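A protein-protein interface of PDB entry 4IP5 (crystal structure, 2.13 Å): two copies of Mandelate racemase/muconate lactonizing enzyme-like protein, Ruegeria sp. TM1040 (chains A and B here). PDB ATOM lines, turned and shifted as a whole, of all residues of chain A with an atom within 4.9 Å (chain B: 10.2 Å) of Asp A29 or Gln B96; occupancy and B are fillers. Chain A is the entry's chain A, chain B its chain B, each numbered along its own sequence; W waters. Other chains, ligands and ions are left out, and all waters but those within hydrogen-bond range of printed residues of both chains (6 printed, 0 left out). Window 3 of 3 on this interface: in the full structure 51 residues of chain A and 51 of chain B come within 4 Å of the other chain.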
ATOM      1  N   SER A  17     -39.365 -21.405   2.476  1.00  0.00           N
ATOM      2  CA  SER A  17     -39.010 -20.231   3.268  1.00  0.00           C
ATOM      3  C   SER A  17     -40.112 -19.830   4.249  1.00  0.00           C
ATOM      4  O   SER A  17     -39.872 -19.010   5.131  1.00  0.00           O
ATOM      5  CB  SER A  17     -38.635 -19.045   2.373  1.00  0.00           C
ATOM      6  OG  SER A  17     -39.750 -18.612   1.609  1.00  0.00           O
ATOM      7  N   LEU A  20     -38.720 -21.373   7.145  1.00  0.00           N
ATOM      8  CA  LEU A  20     -37.254 -21.348   7.094  1.00  0.00           C
ATOM      9  C   LEU A  20     -36.629 -22.750   7.127  1.00  0.00           C
ATOM     10  O   LEU A  20     -35.525 -22.939   7.664  1.00  0.00           O
ATOM     11  CB  LEU A  20     -36.681 -20.471   8.213  1.00  0.00           C
ATOM     12  CG  LEU A  20     -37.176 -19.018   8.215  1.00  0.00           C
ATOM     13  CD1 LEU A  20     -36.740 -18.286   9.485  1.00  0.00           C
ATOM     14  CD2 LEU A  20     -36.707 -18.272   6.967  1.00  0.00           C
ATOM     15  N   ASN A  27     -27.540 -19.185   3.140  1.00  0.00           N
ATOM     16  CA  ASN A  27     -28.846 -19.159   2.494  1.00  0.00           C
ATOM     17  C   ASN A  27     -29.936 -18.997   3.542  1.00  0.00           C
ATOM     18  O   ASN A  27     -30.414 -19.988   4.113  1.00  0.00           O
ATOM     19  CB  ASN A  27     -29.055 -20.463   1.701  1.00  0.00           C
ATOM     20  CG  ASN A  27     -27.823 -20.852   0.883  1.00  0.00           C
ATOM     21  OD1 ASN A  27     -27.439 -20.140  -0.046  1.00  0.00           O
ATOM     22  ND2 ASN A  27     -27.195 -21.968   1.237  1.00  0.00           N
ATOM     23  N   PRO A  28     -30.323 -17.743   3.816  1.00  0.00           N
ATOM     24  CA  PRO A  28     -31.250 -17.442   4.914  1.00  0.00           C
ATOM     25  C   PRO A  28     -32.687 -17.879   4.650  1.00  0.00           C
ATOM     26  O   PRO A  28     -33.395 -18.201   5.595  1.00  0.00           O
ATOM     27  CB  PRO A  28     -31.182 -15.915   5.020  1.00  0.00           C
ATOM     28  CG  PRO A  28     -30.800 -15.464   3.660  1.00  0.00           C
ATOM     29  CD  PRO A  28     -29.889 -16.528   3.107  1.00  0.00           C
ATOM     30  N   ASP A  29     -33.113 -17.889   3.394  1.00  0.00           N
ATOM     31  CA  ASP A  29     -34.507 -18.188   3.084  1.00  0.00           C
ATOM     32  C   ASP A  29     -34.692 -18.997   1.794  1.00  0.00           C
ATOM     33  O   ASP A  29     -35.425 -18.582   0.898  1.00  0.00           O
ATOM     34  CB  ASP A  29     -35.299 -16.883   3.007  1.00  0.00           C
ATOM     35  CG  ASP A  29     -34.683 -15.882   2.043  1.00  0.00           C
ATOM     36  OD1 ASP A  29     -33.565 -16.130   1.530  1.00  0.00           O
ATOM     37  OD2 ASP A  29     -35.319 -14.844   1.790  1.00  0.00           O
ATOM     38  N   PRO A  30     -34.041 -20.166   1.701  1.00  0.00           N
ATOM     39  CA  PRO A  30     -34.130 -20.919   0.448  1.00  0.00           C
ATOM     40  C   PRO A  30     -35.547 -21.407   0.154  1.00  0.00           C
ATOM     41  O   PRO A  30     -36.283 -21.814   1.062  1.00  0.00           O
ATOM     42  CB  PRO A  30     -33.211 -22.118   0.699  1.00  0.00           C
ATOM     43  CG  PRO A  30     -33.232 -22.291   2.190  1.00  0.00           C
ATOM     44  CD  PRO A  30     -33.284 -20.896   2.736  1.00  0.00           C
ATOM     45  N   ASP A  31     -35.915 -21.349  -1.121  1.00  0.00           N
ATOM     46  CA  ASP A  31     -37.150 -21.933  -1.622  1.00  0.00           C
ATOM     47  C   ASP A  31     -36.802 -23.157  -2.444  1.00  0.00           C
ATOM     48  O   ASP A  31     -36.501 -23.046  -3.639  1.00  0.00           O
ATOM     49  CB  ASP A  31     -37.889 -20.932  -2.497  1.00  0.00           C
ATOM     50  CG  ASP A  31     -38.553 -19.841  -1.685  1.00  0.00           C
ATOM     51  OD1 ASP A  31     -39.189 -20.184  -0.658  1.00  0.00           O
ATOM     52  OD2 ASP A  31     -38.425 -18.655  -2.069  1.00  0.00           O
ATOM     53  N   ILE A  54     -32.407 -23.521  -5.061  1.00  0.00           N
ATOM     54  CA  ILE A  54     -33.136 -22.935  -3.939  1.00  0.00           C
ATOM     55  C   ILE A  54     -33.964 -21.707  -4.316  1.00  0.00           C
ATOM     56  O   ILE A  54     -34.140 -20.793  -3.504  1.00  0.00           O
ATOM     57  CB  ILE A  54     -32.207 -22.621  -2.747  1.00  0.00           C
ATOM     58  CG1 ILE A  54     -31.049 -21.708  -3.180  1.00  0.00           C
ATOM     59  CG2 ILE A  54     -31.663 -23.922  -2.141  1.00  0.00           C
ATOM     60  CD1 ILE A  54     -30.226 -21.157  -2.009  1.00  0.00           C
ATOM     61  N   GLY A  55     -34.475 -21.685  -5.542  1.00  0.00           N
ATOM     62  CA  GLY A  55     -35.434 -20.660  -5.927  1.00  0.00           C
ATOM     63  C   GLY A  55     -35.071 -19.906  -7.190  1.00  0.00           C
ATOM     64  O   GLY A  55     -35.077 -20.481  -8.286  1.00  0.00           O
ATOM     65  N   ARG A  56     -34.779 -18.613  -7.039  1.00  0.00           N
ATOM     66  CA  ARG A  56     -34.338 -17.793  -8.158  1.00  0.00           C
ATOM     67  C   ARG A  56     -33.136 -18.458  -8.835  1.00  0.00           C
ATOM     68  O   ARG A  56     -32.219 -18.937  -8.161  1.00  0.00           O
ATOM     69  CB  ARG A  56     -33.968 -16.393  -7.665  1.00  0.00           C
ATOM     70  CG  ARG A  56     -35.165 -15.589  -7.138  1.00  0.00           C
ATOM     71  CD  ARG A  56     -34.749 -14.187  -6.672  1.00  0.00           C
ATOM     72  NE  ARG A  56     -33.760 -14.243  -5.599  1.00  0.00           N
ATOM     73  CZ  ARG A  56     -34.063 -14.441  -4.318  1.00  0.00           C
ATOM     74  NH1 ARG A  56     -35.335 -14.587  -3.940  1.00  0.00           N
ATOM     75  NH2 ARG A  56     -33.095 -14.490  -3.410  1.00  0.00           N
ATOM     76  N   ALA B  67     -31.650 -12.748 -14.945  1.00  0.00           N
ATOM     77  CA  ALA B  67     -31.809 -13.047 -13.528  1.00  0.00           C
ATOM     78  C   ALA B  67     -31.062 -12.014 -12.703  1.00  0.00           C
ATOM     79  O   ALA B  67     -31.568 -11.527 -11.694  1.00  0.00           O
ATOM     80  CB  ALA B  67     -31.289 -14.454 -13.213  1.00  0.00           C
ATOM     81  N   LEU B  68     -29.853 -11.680 -13.141  1.00  0.00           N
ATOM     82  CA  LEU B  68     -29.018 -10.731 -12.418  1.00  0.00           C
ATOM     83  C   LEU B  68     -29.605  -9.332 -12.468  1.00  0.00           C
ATOM     84  O   LEU B  68     -29.335  -8.518 -11.593  1.00  0.00           O
ATOM     85  CB  LEU B  68     -27.606 -10.710 -12.991  1.00  0.00           C
ATOM     86  CG  LEU B  68     -26.771 -11.941 -12.665  1.00  0.00           C
ATOM     87  CD1 LEU B  68     -25.431 -11.839 -13.352  1.00  0.00           C
ATOM     88  CD2 LEU B  68     -26.596 -12.081 -11.151  1.00  0.00           C
ATOM     89  N   ALA B  70     -32.455  -8.290 -11.858  1.00  0.00           N
ATOM     90  CA  ALA B  70     -33.249  -8.018 -10.667  1.00  0.00           C
ATOM     91  C   ALA B  70     -32.424  -7.320  -9.587  1.00  0.00           C
ATOM     92  O   ALA B  70     -32.962  -6.566  -8.788  1.00  0.00           O
ATOM     93  CB  ALA B  70     -33.854  -9.310 -10.124  1.00  0.00           C
ATOM     94  N   LEU B  71     -31.116  -7.566  -9.576  1.00  0.00           N
ATOM     95  CA  LEU B  71     -30.245  -7.028  -8.533  1.00  0.00           C
ATOM     96  C   LEU B  71     -29.689  -5.638  -8.866  1.00  0.00           C
ATOM     97  O   LEU B  71     -29.138  -4.954  -7.999  1.00  0.00           O
ATOM     98  CB  LEU B  71     -29.078  -7.992  -8.288  1.00  0.00           C
ATOM     99  CG  LEU B  71     -29.459  -9.418  -7.903  1.00  0.00           C
ATOM    100  CD1 LEU B  71     -28.216 -10.283  -7.818  1.00  0.00           C
ATOM    101  CD2 LEU B  71     -30.244  -9.421  -6.581  1.00  0.00           C
ATOM    102  N   HIS B  90     -22.809  -7.494  -3.745  1.00  0.00           N
ATOM    103  CA  HIS B  90     -24.257  -7.442  -3.937  1.00  0.00           C
ATOM    104  C   HIS B  90     -24.688  -8.235  -5.178  1.00  0.00           C
ATOM    105  O   HIS B  90     -25.625  -9.049  -5.129  1.00  0.00           O
ATOM    106  CB  HIS B  90     -24.712  -5.982  -4.041  1.00  0.00           C
ATOM    107  CG  HIS B  90     -26.138  -5.816  -4.464  1.00  0.00           C
ATOM    108  ND1 HIS B  90     -27.197  -6.052  -3.616  1.00  0.00           N
ATOM    109  CD2 HIS B  90     -26.678  -5.424  -5.644  1.00  0.00           C
ATOM    110  CE1 HIS B  90     -28.331  -5.825  -4.258  1.00  0.00           C
ATOM    111  NE2 HIS B  90     -28.044  -5.443  -5.491  1.00  0.00           N
ATOM    112  N   VAL B  91     -23.990  -8.022  -6.287  1.00  0.00           N
ATOM    113  CA  VAL B  91     -24.445  -8.590  -7.549  1.00  0.00           C
ATOM    114  C   VAL B  91     -24.131 -10.094  -7.647  1.00  0.00           C
ATOM    115  O   VAL B  91     -24.832 -10.833  -8.339  1.00  0.00           O
ATOM    116  CB  VAL B  91     -23.938  -7.768  -8.785  1.00  0.00           C
ATOM    117  CG1 VAL B  91     -22.477  -8.051  -9.075  1.00  0.00           C
ATOM    118  CG2 VAL B  91     -24.796  -8.061 -10.005  1.00  0.00           C
ATOM    119  N   THR B  92     -23.097 -10.546  -6.938  1.00  0.00           N
ATOM    120  CA  THR B  92     -22.762 -11.972  -6.905  1.00  0.00           C
ATOM    121  C   THR B  92     -23.274 -12.626  -5.621  1.00  0.00           C
ATOM    122  O   THR B  92     -22.975 -13.797  -5.345  1.00  0.00           O
ATOM    123  CB  THR B  92     -21.235 -12.214  -7.009  1.00  0.00           C
ATOM    124  OG1 THR B  92     -20.565 -11.575  -5.910  1.00  0.00           O
ATOM    125  CG2 THR B  92     -20.680 -11.673  -8.331  1.00  0.00           C
ATOM    126  N   GLY B  93     -24.044 -11.870  -4.842  1.00  0.00           N
ATOM    127  CA  GLY B  93     -24.399 -12.285  -3.499  1.00  0.00           C
ATOM    128  C   GLY B  93     -25.820 -12.744  -3.239  1.00  0.00           C
ATOM    129  O   GLY B  93     -26.140 -13.080  -2.106  1.00  0.00           O
ATOM    130  N   ASP B  94     -26.681 -12.756  -4.254  1.00  0.00           N
ATOM    131  CA  ASP B  94     -28.001 -13.371  -4.087  1.00  0.00           C
ATOM    132  C   ASP B  94     -27.762 -14.864  -3.821  1.00  0.00           C
ATOM    133  O   ASP B  94     -27.331 -15.591  -4.713  1.00  0.00           O
ATOM    134  CB  ASP B  94     -28.842 -13.158  -5.350  1.00  0.00           C
ATOM    135  CG  ASP B  94     -30.262 -13.732  -5.244  1.00  0.00           C
ATOM    136  OD1 ASP B  94     -30.484 -14.740  -4.547  1.00  0.00           O
ATOM    137  OD2 ASP B  94     -31.166 -13.177  -5.901  1.00  0.00           O
ATOM    138  N   SER B  95     -28.030 -15.312  -2.595  1.00  0.00           N
ATOM    139  CA  SER B  95     -27.742 -16.696  -2.201  1.00  0.00           C
ATOM    140  C   SER B  95     -28.387 -17.715  -3.136  1.00  0.00           C
ATOM    141  O   SER B  95     -27.811 -18.760  -3.419  1.00  0.00           O
ATOM    142  CB  SER B  95     -28.193 -16.957  -0.772  1.00  0.00           C
ATOM    143  OG  SER B  95     -29.600 -16.903  -0.674  1.00  0.00           O
ATOM    144  N   GLN B  96     -29.576 -17.394  -3.630  1.00  0.00           N
ATOM    145  CA  GLN B  96     -30.268 -18.274  -4.559  1.00  0.00           C
ATOM    146  C   GLN B  96     -29.592 -18.297  -5.941  1.00  0.00           C
ATOM    147  O   GLN B  96     -29.399 -19.371  -6.519  1.00  0.00           O
ATOM    148  CB  GLN B  96     -31.755 -17.905  -4.622  1.00  0.00           C
ATOM    149  CG  GLN B  96     -32.447 -18.128  -3.275  1.00  0.00           C
ATOM    150  CD  GLN B  96     -33.932 -17.826  -3.279  1.00  0.00           C
ATOM    151  OE1 GLN B  96     -34.547 -17.638  -4.335  1.00  0.00           O
ATOM    152  NE2 GLN B  96     -34.527 -17.785  -2.080  1.00  0.00           N
ATOM    153  N   LEU B  97     -29.200 -17.134  -6.461  1.00  0.00           N
ATOM    154  CA  LEU B  97     -28.445 -17.116  -7.723  1.00  0.00           C
ATOM    155  C   LEU B  97     -27.050 -17.732  -7.567  1.00  0.00           C
ATOM    156  O   LEU B  97     -26.530 -18.345  -8.512  1.00  0.00           O
ATOM    157  CB  LEU B  97     -28.363 -15.701  -8.322  1.00  0.00           C
ATOM    158  CG  LEU B  97     -29.721 -15.146  -8.756  1.00  0.00           C
ATOM    159  CD1 LEU B  97     -29.585 -13.802  -9.499  1.00  0.00           C
ATOM    160  CD2 LEU B  97     -30.471 -16.182  -9.601  1.00  0.00           C
ATOM    161  N   ARG B  98     -26.454 -17.578  -6.381  1.00  0.00           N
ATOM    162  CA  ARG B  98     -25.171 -18.217  -6.055  1.00  0.00           C
ATOM    163  C   ARG B  98     -25.215 -19.730  -6.205  1.00  0.00           C
ATOM    164  O   ARG B  98     -24.228 -20.352  -6.601  1.00  0.00           O
ATOM    165  CB  ARG B  98     -24.738 -17.898  -4.620  1.00  0.00           C
ATOM    166  CG  ARG B  98     -24.171 -16.516  -4.452  1.00  0.00           C
ATOM    167  CD  ARG B  98     -23.580 -16.327  -3.063  1.00  0.00           C
ATOM    168  NE  ARG B  98     -22.300 -17.011  -2.874  1.00  0.00           N
ATOM    169  CZ  ARG B  98     -21.129 -16.561  -3.329  1.00  0.00           C
ATOM    170  NH1 ARG B  98     -21.063 -15.431  -4.033  1.00  0.00           N
ATOM    171  NH2 ARG B  98     -20.019 -17.251  -3.085  1.00  0.00           N
ATOM    172  N   TRP B  99     -26.355 -20.318  -5.859  1.00  0.00           N
ATOM    173  CA  TRP B  99     -26.527 -21.766  -5.921  1.00  0.00           C
ATOM    174  C   TRP B  99     -26.257 -22.296  -7.324  1.00  0.00           C
ATOM    175  O   TRP B  99     -25.798 -23.429  -7.499  1.00  0.00           O
ATOM    176  CB  TRP B  99     -27.949 -22.148  -5.512  1.00  0.00           C
ATOM    177  CG  TRP B  99     -28.048 -23.589  -5.212  1.00  0.00           C
ATOM    178  CD1 TRP B  99     -28.255 -24.602  -6.098  1.00  0.00           C
ATOM    179  CD2 TRP B  99     -27.903 -24.198  -3.922  1.00  0.00           C
ATOM    180  NE1 TRP B  99     -28.263 -25.812  -5.437  1.00  0.00           N
ATOM    181  CE2 TRP B  99     -28.054 -25.588  -4.099  1.00  0.00           C
ATOM    182  CE3 TRP B  99     -27.695 -23.695  -2.631  1.00  0.00           C
ATOM    183  CZ2 TRP B  99     -27.978 -26.487  -3.035  1.00  0.00           C
ATOM    184  CZ3 TRP B  99     -27.616 -24.592  -1.574  1.00  0.00           C
ATOM    185  CH2 TRP B  99     -27.764 -25.969  -1.782  1.00  0.00           C
ATOM    186  N   ILE B 100     -26.550 -21.465  -8.322  1.00  0.00           N
ATOM    187  CA  ILE B 100     -26.381 -21.828  -9.730  1.00  0.00           C
ATOM    188  C   ILE B 100     -24.883 -21.837 -10.086  1.00  0.00           C
ATOM    189  O   ILE B 100     -24.466 -22.402 -11.105  1.00  0.00           O
ATOM    190  CB  ILE B 100     -27.176 -20.845 -10.634  1.00  0.00           C
ATOM    191  CG1 ILE B 100     -28.590 -20.655 -10.079  1.00  0.00           C
ATOM    192  CG2 ILE B 100     -27.245 -21.333 -12.070  1.00  0.00           C
ATOM    193  CD1 ILE B 100     -29.409 -21.950  -9.999  1.00  0.00           C
ATOM    194  N   GLY B 101     -24.085 -21.212  -9.224  1.00  0.00           N
ATOM    195  CA  GLY B 101     -22.635 -21.183  -9.364  1.00  0.00           C
ATOM    196  C   GLY B 101     -21.978 -22.003  -8.267  1.00  0.00           C
ATOM    197  O   GLY B 101     -21.977 -23.225  -8.345  1.00  0.00           O
ATOM    198  N   PRO B 102     -21.400 -21.340  -7.243  1.00  0.00           N
ATOM    199  CA  PRO B 102     -21.212 -19.885  -7.132  1.00  0.00           C
ATOM    200  C   PRO B 102     -20.003 -19.400  -7.935  1.00  0.00           C
ATOM    201  O   PRO B 102     -18.988 -20.100  -8.021  1.00  0.00           O
ATOM    202  CB  PRO B 102     -20.964 -19.667  -5.624  1.00  0.00           C
ATOM    203  CG  PRO B 102     -21.305 -21.015  -4.950  1.00  0.00           C
ATOM    204  CD  PRO B 102     -21.013 -22.033  -6.004  1.00  0.00           C
ATOM    205  N   ASP B 103     -20.116 -18.206  -8.513  1.00  0.00           N
ATOM    206  CA  ASP B 103     -18.996 -17.603  -9.220  1.00  0.00           C
ATOM    207  C   ASP B 103     -18.387 -18.583 -10.239  1.00  0.00           C
ATOM    208  O   ASP B 103     -17.175 -18.764 -10.293  1.00  0.00           O
ATOM    209  CB  ASP B 103     -17.936 -17.131  -8.214  1.00  0.00           C
ATOM    210  CG  ASP B 103     -18.400 -15.925  -7.390  1.00  0.00           C
ATOM    211  OD1 ASP B 103     -19.554 -15.487  -7.565  1.00  0.00           O
ATOM    212  OD2 ASP B 103     -17.619 -15.417  -6.560  1.00  0.00           O
ATOM    213  N   ILE B 107     -23.878 -18.303 -14.615  1.00  0.00           N
ATOM    214  CA  ILE B 107     -24.198 -17.182 -13.736  1.00  0.00           C
ATOM    215  C   ILE B 107     -23.006 -16.230 -13.585  1.00  0.00           C
ATOM    216  O   ILE B 107     -23.191 -15.035 -13.376  1.00  0.00           O
ATOM    217  CB  ILE B 107     -24.720 -17.643 -12.344  1.00  0.00           C
ATOM    218  CG1 ILE B 107     -25.383 -16.476 -11.602  1.00  0.00           C
ATOM    219  CG2 ILE B 107     -23.596 -18.223 -11.496  1.00  0.00           C
ATOM    220  CD1 ILE B 107     -26.628 -15.915 -12.296  1.00  0.00           C
HETATM  221  O   HOH W   1     -25.792 -20.263  -2.157  1.00  0.00           O
HETATM  222  O   HOH W   2     -32.552 -11.186  -4.044  1.00  0.00           O
HETATM  223  O   HOH W   3     -37.006 -17.013  -0.496  1.00  0.00           O
HETATM  224  O   HOH W   4     -31.982 -17.969   0.367  1.00  0.00           O
HETATM  225  O   HOH W   5     -37.299 -17.734  -4.261  1.00  0.00           O
HETATM  226  O   HOH W   6     -31.370 -21.275  -6.715  1.00  0.00           O
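Water W3 lies within hydrogen-bond range of O of Asp A29 (2.6 Å), OD2 of Asp A31 (2.7 Å) and NE2 of Gln B96 (3.0 Å).
Water W5 bridges OD2 of Asp A31 (2.6 Å) and OE1 of Gln B96 (2.8 Å).
Water W1 bridges OD1 of Asn A27 (2.7 Å) and O of Ser B95 (2.8 Å).
Water W4 lies within hydrogen-bond range of OD1 of Asp A29 (2.7 Å) and OG of Ser B95 (2.8 Å).
Water W6 lies within hydrogen-bond range of the backbone carbonyl oxygen (O) of Gln B96 (2.7 Å), the backbone carbonyl oxygen (O) of Arg A56 (2.9 Å), the backbone NH (N) of Ile A54 (3.0 Å) and the backbone NH (N) of Gly A55 (3.3 Å).
Water W2 lies within hydrogen-bond range of the side-chain carboxylate of Asp B94 (3.1 Å) and the guanidinium group of Arg A56 (3.4 Å).
Among the printed residues, merely in contact across the chains: Asn A27 with Ser B95 (3.4 Å), Gly A55 with Gln B96 (3.5 Å), Arg A56 with Leu B97 (3.6 Å), Ile A54 with Trp B99 (3.6 Å), Ile A54 with Ser B95 (3.7 Å), Pro A28 with Ser B95 (3.8 Å), Asn A27 with Trp B99 (3.9 Å) and Asp A31 with Gln B96 (3.9 Å).
The side-chain carboxylate of Asp A31 is in hydrogen-bond range of the side-chain hydroxyl of Ser A17 (2.8 Å).
The backbone carbonyl oxygen of Asp A31 is in hydrogen-bond range of the backbone NH of Gly A55 (3.1 Å).
The side-chain carboxylate of Asp B94 is in hydrogen-bond range of the backbone NH of Leu B97 (3.3 Å).
The backbone NH of Asp A31 is in hydrogen-bond range of the backbone carbonyl oxygen of Ile A54, at 3.0 Å.
OD1 of Asp B94 is in hydrogen-bond range of N of Gln B96.
Of the 19 printed residues of chain B, 5 touch a printed residue of chain A.
Printed residues of chain B that touch a printed residue of chain A: Asp B94, Ser B95, Gln B96, Leu B97 and Trp B99.
Hydrophobic or aromatic side chains of chain B that line the printed part of chain A: Leu B97 and Trp B99.
Of the 10 printed residues of chain A, 7 touch a printed residue of chain B.
Printed residues of chain A that touch a printed residue of chain B: Asn A27, Pro A28, Asp A29, Asp A31, Ile A54, Gly A55 and Arg A56.
Among the printed residues, 12 pairs touch across the chains.
Among the printed residues, Asp or Glu carboxylates within 4 Å of a Lys or Arg side-chain nitrogen of the other chain: Arg A56 with Asp B94.
The backbone carbonyl oxygen of Ile A54 sits close to the side-chain amide oxygen of Gln B96, 3.3 Å away.
O of Asp A29 sits at hydrogen-bond distance from NE2 of Gln B96 (3.2 Å).
NE of Arg A56 is in salt-bridge range of OD2 of Asp B94.
The backbone NH (N) of Arg A56 is in hydrogen-bond range of the side-chain amide oxygen (OE1) of Gln B96 (2.9 Å).
No position is printed for both chains.
Of the 12 pairs that touch across the chains among the printed residues, none has its exchanged pair printed and touching as well.
Of chain A, only Asp A29, Asp A31, Ile A54, Gly A55 and Arg A56 come within 4 Å of Gln B96.
Ser A17 touches none of the printed residues of chain B.
Pro A28 touches just one residue of chain B: Ser B95.
No residue of chain B comes within 4 Å of Pro A30.
Asp A31 touches one residue of chain B.
Of the printed residues of chain B, Asn A27 touches Ser B95 and Trp B99.
Of the printed residues of chain A, Asp B94 touches Arg A56.
Of the printed residues of chain A, Trp B99 touches Asn A27 (3.9 Å) and Ile A54 (3.6 Å).
Asp B103 touches none of the printed residues of chain A.
Ile B107 touches none of the printed residues of chain A.
The nearest residue of chain A that does not touch Gln B96 is Pro A30 (4.05 Å).
The nearest printed residue of chain B that does not touch Asn A27 is Gln B96 (5.0 Å).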
